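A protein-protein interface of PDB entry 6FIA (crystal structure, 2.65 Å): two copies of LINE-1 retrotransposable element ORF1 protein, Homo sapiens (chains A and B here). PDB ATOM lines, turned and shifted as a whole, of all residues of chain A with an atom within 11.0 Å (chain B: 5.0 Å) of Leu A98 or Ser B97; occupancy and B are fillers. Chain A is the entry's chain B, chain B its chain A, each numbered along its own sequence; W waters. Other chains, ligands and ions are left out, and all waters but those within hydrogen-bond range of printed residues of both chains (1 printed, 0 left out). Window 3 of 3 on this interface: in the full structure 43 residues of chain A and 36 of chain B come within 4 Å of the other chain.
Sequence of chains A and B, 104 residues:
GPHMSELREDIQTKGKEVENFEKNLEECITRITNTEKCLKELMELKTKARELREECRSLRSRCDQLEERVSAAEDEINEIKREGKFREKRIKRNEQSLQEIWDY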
ATOM      1  N   ARG A  90       9.092 -10.229  21.661  1.00  0.00           N
ATOM      2  CA  ARG A  90       9.490 -11.086  20.548  1.00  0.00           C
ATOM      3  C   ARG A  90      10.878 -11.690  20.700  1.00  0.00           C
ATOM      4  O   ARG A  90      11.034 -12.894  20.482  1.00  0.00           O
ATOM      5  CB  ARG A  90       9.353 -10.339  19.245  1.00  0.00           C
ATOM      6  CG  ARG A  90       7.870 -10.111  18.882  1.00  0.00           C
ATOM      7  CD  ARG A  90       7.720  -9.049  17.829  1.00  0.00           C
ATOM      8  NE  ARG A  90       8.091  -9.551  16.509  1.00  0.00           N
ATOM      9  CZ  ARG A  90       8.547  -8.793  15.518  1.00  0.00           C
ATOM     10  NH1 ARG A  90       8.745  -7.496  15.703  1.00  0.00           N
ATOM     11  NH2 ARG A  90       8.815  -9.329  14.338  1.00  0.00           N
ATOM     12  N   ILE A  91      11.878 -10.883  21.124  1.00  0.00           N
ATOM     13  CA  ILE A  91      13.224 -11.388  21.396  1.00  0.00           C
ATOM     14  C   ILE A  91      13.148 -12.448  22.508  1.00  0.00           C
ATOM     15  O   ILE A  91      13.684 -13.553  22.349  1.00  0.00           O
ATOM     16  CB  ILE A  91      14.229 -10.250  21.752  1.00  0.00           C
ATOM     17  CG1 ILE A  91      14.363  -9.233  20.599  1.00  0.00           C
ATOM     18  CG2 ILE A  91      15.614 -10.820  22.144  1.00  0.00           C
ATOM     19  CD1 ILE A  91      15.014  -7.914  20.991  1.00  0.00           C
ATOM     20  N   LYS A  92      12.442 -12.130  23.613  1.00  0.00           N
ATOM     21  CA  LYS A  92      12.312 -13.060  24.728  1.00  0.00           C
ATOM     22  C   LYS A  92      11.704 -14.408  24.301  1.00  0.00           C
ATOM     23  O   LYS A  92      12.224 -15.451  24.690  1.00  0.00           O
ATOM     24  CB  LYS A  92      11.550 -12.431  25.890  1.00  0.00           C
ATOM     25  CG  LYS A  92      11.814 -13.140  27.211  1.00  0.00           C
ATOM     26  CD  LYS A  92      11.070 -12.477  28.339  1.00  0.00           C
ATOM     27  CE  LYS A  92      11.094 -13.325  29.590  1.00  0.00           C
ATOM     28  NZ  LYS A  92      10.343 -12.682  30.703  1.00  0.00           N
ATOM     29  N   ARG A  93      10.666 -14.381  23.438  1.00  0.00           N
ATOM     30  CA  ARG A  93      10.009 -15.576  22.873  1.00  0.00           C
ATOM     31  C   ARG A  93      11.026 -16.400  22.074  1.00  0.00           C
ATOM     32  O   ARG A  93      11.110 -17.611  22.251  1.00  0.00           O
ATOM     33  CB  ARG A  93       8.886 -15.131  21.944  1.00  0.00           C
ATOM     34  CG  ARG A  93       7.566 -15.803  22.167  1.00  0.00           C
ATOM     35  CD  ARG A  93       6.601 -15.595  20.975  1.00  0.00           C
ATOM     36  NE  ARG A  93       6.459 -14.190  20.544  1.00  0.00           N
ATOM     37  CZ  ARG A  93       5.629 -13.311  21.107  1.00  0.00           C
ATOM     38  NH1 ARG A  93       4.891 -13.658  22.153  1.00  0.00           N
ATOM     39  NH2 ARG A  93       5.553 -12.070  20.643  1.00  0.00           N
ATOM     40  N   ASN A  94      11.821 -15.734  21.216  1.00  0.00           N
ATOM     41  CA  ASN A  94      12.870 -16.371  20.411  1.00  0.00           C
ATOM     42  C   ASN A  94      13.928 -17.010  21.270  1.00  0.00           C
ATOM     43  O   ASN A  94      14.326 -18.138  20.994  1.00  0.00           O
ATOM     44  CB  ASN A  94      13.480 -15.390  19.426  1.00  0.00           C
ATOM     45  CG  ASN A  94      12.552 -14.974  18.305  1.00  0.00           C
ATOM     46  OD1 ASN A  94      11.494 -15.582  18.076  1.00  0.00           O
ATOM     47  ND2 ASN A  94      12.939 -13.934  17.569  1.00  0.00           N
ATOM     48  N   GLU A  95      14.334 -16.330  22.361  1.00  0.00           N
ATOM     49  CA  GLU A  95      15.315 -16.858  23.330  1.00  0.00           C
ATOM     50  C   GLU A  95      14.767 -18.113  23.998  1.00  0.00           C
ATOM     51  O   GLU A  95      15.503 -19.077  24.155  1.00  0.00           O
ATOM     52  CB  GLU A  95      15.667 -15.800  24.408  1.00  0.00           C
ATOM     53  CG  GLU A  95      16.545 -14.661  23.911  1.00  0.00           C
ATOM     54  CD  GLU A  95      16.786 -13.529  24.900  1.00  0.00           C
ATOM     55  OE1 GLU A  95      15.834 -13.166  25.632  1.00  0.00           O
ATOM     56  OE2 GLU A  95      17.920 -12.982  24.918  1.00  0.00           O
ATOM     57  N   GLN A  96      13.460 -18.104  24.386  1.00  0.00           N
ATOM     58  CA  GLN A  96      12.805 -19.258  25.009  1.00  0.00           C
ATOM     59  C   GLN A  96      12.708 -20.441  24.051  1.00  0.00           C
ATOM     60  O   GLN A  96      12.965 -21.573  24.456  1.00  0.00           O
ATOM     61  CB  GLN A  96      11.440 -18.901  25.605  1.00  0.00           C
ATOM     62  CG  GLN A  96      11.545 -18.058  26.889  1.00  0.00           C
ATOM     63  CD  GLN A  96      10.306 -17.201  27.224  1.00  0.00           C
ATOM     64  OE1 GLN A  96       9.376 -17.018  26.411  1.00  0.00           O
ATOM     65  NE2 GLN A  96      10.307 -16.595  28.419  1.00  0.00           N
ATOM     66  N   SER A  97      12.382 -20.177  22.775  1.00  0.00           N
ATOM     67  CA  SER A  97      12.314 -21.207  21.744  1.00  0.00           C
ATOM     68  C   SER A  97      13.678 -21.871  21.584  1.00  0.00           C
ATOM     69  O   SER A  97      13.745 -23.095  21.524  1.00  0.00           O
ATOM     70  CB  SER A  97      11.877 -20.602  20.418  1.00  0.00           C
ATOM     71  OG  SER A  97      10.484 -20.374  20.420  1.00  0.00           O
ATOM     72  N   LEU A  98      14.771 -21.069  21.532  1.00  0.00           N
ATOM     73  CA  LEU A  98      16.124 -21.583  21.378  1.00  0.00           C
ATOM     74  C   LEU A  98      16.587 -22.385  22.575  1.00  0.00           C
ATOM     75  O   LEU A  98      17.224 -23.416  22.391  1.00  0.00           O
ATOM     76  CB  LEU A  98      17.114 -20.463  21.067  1.00  0.00           C
ATOM     77  CG  LEU A  98      17.065 -19.883  19.650  1.00  0.00           C
ATOM     78  CD1 LEU A  98      17.764 -18.571  19.601  1.00  0.00           C
ATOM     79  CD2 LEU A  98      17.613 -20.878  18.603  1.00  0.00           C
ATOM     80  N   GLN A  99      16.270 -21.938  23.799  1.00  0.00           N
ATOM     81  CA  GLN A  99      16.596 -22.675  25.013  1.00  0.00           C
ATOM     82  C   GLN A  99      15.888 -24.017  24.989  1.00  0.00           C
ATOM     83  O   GLN A  99      16.523 -25.031  25.279  1.00  0.00           O
ATOM     84  CB  GLN A  99      16.229 -21.862  26.279  1.00  0.00           C
ATOM     85  CG  GLN A  99      17.021 -22.251  27.537  1.00  0.00           C
ATOM     86  CD  GLN A  99      18.541 -22.091  27.380  1.00  0.00           C
ATOM     87  OE1 GLN A  99      19.232 -22.933  26.772  1.00  0.00           O
ATOM     88  NE2 GLN A  99      19.100 -21.027  27.969  1.00  0.00           N
ATOM     89  N   GLU A 100      14.629 -24.061  24.516  1.00  0.00           N
ATOM     90  CA  GLU A 100      13.894 -25.322  24.410  1.00  0.00           C
ATOM     91  C   GLU A 100      14.508 -26.296  23.407  1.00  0.00           C
ATOM     92  O   GLU A 100      14.568 -27.500  23.689  1.00  0.00           O
ATOM     93  CB  GLU A 100      12.424 -25.075  24.124  1.00  0.00           C
ATOM     94  CG  GLU A 100      11.679 -24.587  25.355  1.00  0.00           C
ATOM     95  CD  GLU A 100      10.332 -23.945  25.096  1.00  0.00           C
ATOM     96  OE1 GLU A 100       9.503 -24.567  24.391  1.00  0.00           O
ATOM     97  OE2 GLU A 100      10.087 -22.841  25.638  1.00  0.00           O
ATOM     98  N   ILE A 101      15.008 -25.769  22.260  1.00  0.00           N
ATOM     99  CA  ILE A 101      15.670 -26.550  21.221  1.00  0.00           C
ATOM    100  C   ILE A 101      16.969 -27.152  21.770  1.00  0.00           C
ATOM    101  O   ILE A 101      17.182 -28.358  21.642  1.00  0.00           O
ATOM    102  CB  ILE A 101      15.898 -25.676  19.933  1.00  0.00           C
ATOM    103  CG1 ILE A 101      14.588 -25.459  19.190  1.00  0.00           C
ATOM    104  CG2 ILE A 101      16.960 -26.260  18.996  1.00  0.00           C
ATOM    105  CD1 ILE A 101      14.509 -24.193  18.405  1.00  0.00           C
ATOM    106  N   TRP A 102      17.803 -26.315  22.414  1.00  0.00           N
ATOM    107  CA  TRP A 102      19.123 -26.694  22.931  1.00  0.00           C
ATOM    108  C   TRP A 102      19.064 -27.530  24.188  1.00  0.00           C
ATOM    109  O   TRP A 102      20.024 -28.241  24.484  1.00  0.00           O
ATOM    110  CB  TRP A 102      20.037 -25.465  23.102  1.00  0.00           C
ATOM    111  CG  TRP A 102      20.589 -24.975  21.786  1.00  0.00           C
ATOM    112  CD1 TRP A 102      20.203 -23.852  21.109  1.00  0.00           C
ATOM    113  CD2 TRP A 102      21.467 -25.705  20.890  1.00  0.00           C
ATOM    114  NE1 TRP A 102      20.806 -23.818  19.861  1.00  0.00           N
ATOM    115  CE2 TRP A 102      21.613 -24.924  19.718  1.00  0.00           C
ATOM    116  CE3 TRP A 102      22.106 -26.968  20.949  1.00  0.00           C
ATOM    117  CZ2 TRP A 102      22.444 -25.319  18.650  1.00  0.00           C
ATOM    118  CZ3 TRP A 102      22.913 -27.371  19.881  1.00  0.00           C
ATOM    119  CH2 TRP A 102      23.070 -26.558  18.747  1.00  0.00           C
ATOM    120  N   ASP A 103      17.929 -27.511  24.895  1.00  0.00           N
ATOM    121  CA  ASP A 103      17.743 -28.349  26.082  1.00  0.00           C
ATOM    122  C   ASP A 103      17.218 -29.731  25.714  1.00  0.00           C
ATOM    123  O   ASP A 103      17.422 -30.685  26.467  1.00  0.00           O
ATOM    124  CB  ASP A 103      16.829 -27.659  27.126  1.00  0.00           C
ATOM    125  CG  ASP A 103      17.534 -26.603  27.947  1.00  0.00           C
ATOM    126  OD1 ASP A 103      18.794 -26.633  28.006  1.00  0.00           O
ATOM    127  OD2 ASP A 103      16.840 -25.696  28.472  1.00  0.00           O
ATOM    128  N   TYR A 104      16.538 -29.823  24.560  1.00  0.00           N
ATOM    129  CA  TYR A 104      15.915 -31.021  24.031  1.00  0.00           C
ATOM    130  C   TYR A 104      16.961 -32.079  23.712  1.00  0.00           C
ATOM    131  O   TYR A 104      16.895 -33.146  24.343  1.00  0.00           O
ATOM    132  CB  TYR A 104      15.070 -30.667  22.798  1.00  0.00           C
ATOM    133  CG  TYR A 104      14.234 -31.807  22.297  1.00  0.00           C
ATOM    134  CD1 TYR A 104      13.008 -32.115  22.885  1.00  0.00           C
ATOM    135  CD2 TYR A 104      14.664 -32.596  21.232  1.00  0.00           C
ATOM    136  CE1 TYR A 104      12.232 -33.191  22.429  1.00  0.00           C
ATOM    137  CE2 TYR A 104      13.893 -33.665  20.760  1.00  0.00           C
ATOM    138  CZ  TYR A 104      12.682 -33.964  21.364  1.00  0.00           C
ATOM    139  OH  TYR A 104      11.949 -35.035  20.907  1.00  0.00           O
ATOM    140  OXT TYR A 104      17.888 -31.794  22.913  1.00  0.00           O
ATOM    141  N   ARG B  93      23.037 -13.020  19.413  1.00  0.00           N
ATOM    142  CA  ARG B  93      23.137 -14.327  20.089  1.00  0.00           C
ATOM    143  C   ARG B  93      22.141 -15.318  19.467  1.00  0.00           C
ATOM    144  O   ARG B  93      22.505 -16.447  19.185  1.00  0.00           O
ATOM    145  CB  ARG B  93      22.815 -14.160  21.569  1.00  0.00           C
ATOM    146  CG  ARG B  93      23.765 -14.856  22.522  1.00  0.00           C
ATOM    147  CD  ARG B  93      23.251 -14.910  23.973  1.00  0.00           C
ATOM    148  NE  ARG B  93      22.650 -13.649  24.463  1.00  0.00           N
ATOM    149  CZ  ARG B  93      23.331 -12.666  25.047  1.00  0.00           C
ATOM    150  NH1 ARG B  93      24.646 -12.755  25.190  1.00  0.00           N
ATOM    151  NH2 ARG B  93      22.702 -11.584  25.488  1.00  0.00           N
ATOM    152  N   ASN B  94      20.884 -14.868  19.222  1.00  0.00           N
ATOM    153  CA  ASN B  94      19.835 -15.684  18.613  1.00  0.00           C
ATOM    154  C   ASN B  94      20.187 -16.093  17.193  1.00  0.00           C
ATOM    155  O   ASN B  94      19.983 -17.249  16.829  1.00  0.00           O
ATOM    156  CB  ASN B  94      18.503 -14.969  18.668  1.00  0.00           C
ATOM    157  CG  ASN B  94      17.901 -14.874  20.058  1.00  0.00           C
ATOM    158  OD1 ASN B  94      18.355 -15.490  21.001  1.00  0.00           O
ATOM    159  ND2 ASN B  94      16.825 -14.130  20.205  1.00  0.00           N
ATOM    160  N   GLU B  95      20.781 -15.171  16.416  1.00  0.00           N
ATOM    161  CA  GLU B  95      21.266 -15.420  15.047  1.00  0.00           C
ATOM    162  C   GLU B  95      22.355 -16.512  15.061  1.00  0.00           C
ATOM    163  O   GLU B  95      22.315 -17.438  14.233  1.00  0.00           O
ATOM    164  CB  GLU B  95      21.799 -14.110  14.402  1.00  0.00           C
ATOM    165  CG  GLU B  95      20.703 -13.117  14.031  1.00  0.00           C
ATOM    166  CD  GLU B  95      21.138 -11.760  13.497  1.00  0.00           C
ATOM    167  OE1 GLU B  95      22.166 -11.222  13.968  1.00  0.00           O
ATOM    168  OE2 GLU B  95      20.410 -11.206  12.644  1.00  0.00           O
ATOM    169  N   GLN B  96      23.299 -16.428  16.046  1.00  0.00           N
ATOM    170  CA  GLN B  96      24.390 -17.405  16.196  1.00  0.00           C
ATOM    171  C   GLN B  96      23.863 -18.755  16.611  1.00  0.00           C
ATOM    172  O   GLN B  96      24.339 -19.764  16.101  1.00  0.00           O
ATOM    173  CB  GLN B  96      25.460 -16.903  17.172  1.00  0.00           C
ATOM    174  CG  GLN B  96      26.311 -15.752  16.589  1.00  0.00           C
ATOM    175  CD  GLN B  96      27.003 -14.875  17.623  1.00  0.00           C
ATOM    176  OE1 GLN B  96      26.720 -14.923  18.829  1.00  0.00           O
ATOM    177  NE2 GLN B  96      27.900 -14.008  17.157  1.00  0.00           N
ATOM    178  N   SER B  97      22.848 -18.784  17.521  1.00  0.00           N
ATOM    179  CA  SER B  97      22.207 -20.028  17.976  1.00  0.00           C
ATOM    180  C   SER B  97      21.542 -20.744  16.825  1.00  0.00           C
ATOM    181  O   SER B  97      21.679 -21.952  16.723  1.00  0.00           O
ATOM    182  CB  SER B  97      21.176 -19.746  19.051  1.00  0.00           C
ATOM    183  OG  SER B  97      21.786 -19.603  20.312  1.00  0.00           O
ATOM    184  N   LEU B  98      20.833 -19.994  15.945  1.00  0.00           N
ATOM    185  CA  LEU B  98      20.193 -20.554  14.763  1.00  0.00           C
ATOM    186  C   LEU B  98      21.218 -21.117  13.781  1.00  0.00           C
ATOM    187  O   LEU B  98      21.038 -22.235  13.304  1.00  0.00           O
ATOM    188  CB  LEU B  98      19.291 -19.523  14.075  1.00  0.00           C
ATOM    189  CG  LEU B  98      17.943 -19.318  14.738  1.00  0.00           C
ATOM    190  CD1 LEU B  98      17.322 -17.992  14.323  1.00  0.00           C
ATOM    191  CD2 LEU B  98      17.001 -20.480  14.425  1.00  0.00           C
ATOM    192  N   GLN B  99      22.308 -20.368  13.518  1.00  0.00           N
ATOM    193  CA  GLN B  99      23.366 -20.815  12.622  1.00  0.00           C
ATOM    194  C   GLN B  99      23.969 -22.133  13.112  1.00  0.00           C
ATOM    195  O   GLN B  99      24.226 -23.018  12.289  1.00  0.00           O
ATOM    196  CB  GLN B  99      24.446 -19.716  12.450  1.00  0.00           C
ATOM    197  CG  GLN B  99      25.160 -19.725  11.089  1.00  0.00           C
ATOM    198  CD  GLN B  99      24.225 -19.982   9.915  1.00  0.00           C
ATOM    199  OE1 GLN B  99      24.325 -21.008   9.216  1.00  0.00           O
ATOM    200  NE2 GLN B  99      23.272 -19.073   9.694  1.00  0.00           N
ATOM    201  N   GLU B 100      24.128 -22.283  14.466  1.00  0.00           N
ATOM    202  CA  GLU B 100      24.665 -23.495  15.115  1.00  0.00           C
ATOM    203  C   GLU B 100      23.734 -24.682  14.933  1.00  0.00           C
ATOM    204  O   GLU B 100      24.220 -25.803  14.807  1.00  0.00           O
ATOM    205  CB  GLU B 100      24.951 -23.255  16.596  1.00  0.00           C
ATOM    206  CG  GLU B 100      26.251 -22.525  16.829  1.00  0.00           C
ATOM    207  CD  GLU B 100      26.425 -21.954  18.221  1.00  0.00           C
ATOM    208  OE1 GLU B 100      26.241 -22.703  19.210  1.00  0.00           O
ATOM    209  OE2 GLU B 100      26.789 -20.760  18.319  1.00  0.00           O
ATOM    210  N   ILE B 101      22.401 -24.442  14.906  1.00  0.00           N
ATOM    211  CA  ILE B 101      21.401 -25.472  14.626  1.00  0.00           C
ATOM    212  C   ILE B 101      21.556 -25.923  13.155  1.00  0.00           C
ATOM    213  O   ILE B 101      21.693 -27.104  12.915  1.00  0.00           O
ATOM    214  CB  ILE B 101      19.945 -25.003  14.959  1.00  0.00           C
ATOM    215  CG1 ILE B 101      19.731 -24.820  16.478  1.00  0.00           C
ATOM    216  CG2 ILE B 101      18.897 -25.965  14.373  1.00  0.00           C
ATOM    217  CD1 ILE B 101      18.582 -23.924  16.822  1.00  0.00           C
HETATM  218  O   HOH W   1      19.822 -13.706  23.132  1.00  0.00           O
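The backbone carbonyl oxygen (O) of Arg B93 lies within hydrogen-bond range of the side-chain hydroxyl (OG) of Ser B97 (3.4 Å).
Ile A91 touches Asn B94 (O to ND2, 3.8 Å).
Asn B94 touches Asn A94 (ND2 to CB, 3.7 Å).
Asn B94 touches Glu A95.
Leu A98 touches Asn B94 (CD1 to OD1, 3.4 Å).
Leu A98 touches Ser B97.
CD2 of Leu A98 touches CD1 of Ile B101, at 3.7 Å.
Ile A101 touches Ile B101 (CG2 to CD1, 3.6 Å).
Trp A102 touches Ser B97 (NE1 to O, 3.8 Å).
CZ2 of Trp A102 touches CB of Glu B100 (3.8 Å).
Trp A102 touches Ile B101 (CZ2 to CG1, 3.5 Å).
Leu A98 touches three residues of chain B.
Of chain A, only Ile A91, Asn A94, Glu A95 and Leu A98 come within 4 Å of Asn B94.
No residue of chain A comes within 4 Å of Leu B98.
Of chain A, only Trp A102 comes within 4 Å of Glu B100.
Of the printed residues of chain B, Asn A94 touches Asn B94.
Of the printed residues of chain B, Ile A91 touches Asn B94.
Of the printed residues of chain B, Glu A95 touches Asn B94 (3.5 Å).
Of the printed residues of chain B, Trp A102 touches Ser B97 (3.8 Å), Glu B100 (3.8 Å) and Ile B101 (3.5 Å).
Printed residues of chain B within 4 Å of Ile A101: Ile B101 (3.6 Å).
The nearest residue of chain B that does not touch Leu A98 is Leu B98 (4.2 Å).
The nearest printed residue of chain B that does not touch Ile A101 is Leu B98 (6.0 Å).
Of the 9 printed residues of chain B, 4 touch a printed residue of chain A.
Printed residues of chain B that touch a printed residue of chain A: Asn B94, Ser B97, Glu B100 and Ile B101.
Hydrophobic or aromatic side chains of chain B that line the printed part of chain A: Ile B101.
Asn B94 touches its own counterpart, Asn A94.
Leu A98 touches Asn B94, but with the chains exchanged Asn A94 does not touch Leu B98 (6.8 Å).
Leu A98 touches Ser B97, but with the chains exchanged Ser A97 does not touch Leu B98 (7.9 Å).
Leu A98 touches Ile B101, but with the chains exchanged Ile A101 does not touch Leu B98 (6.0 Å).
Positions printed for both chains: 93, 94, 95, 96, 97, 98, 99, 100 and 101.
Water W1 lies within hydrogen-bond range of the side-chain carboxylate (OE2) of Glu A95 (2.7 Å), the guanidinium group (NE) of Arg B93 (3.1 Å) and the side-chain amide oxygen (OD1) of Asn B94 (3.1 Å).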
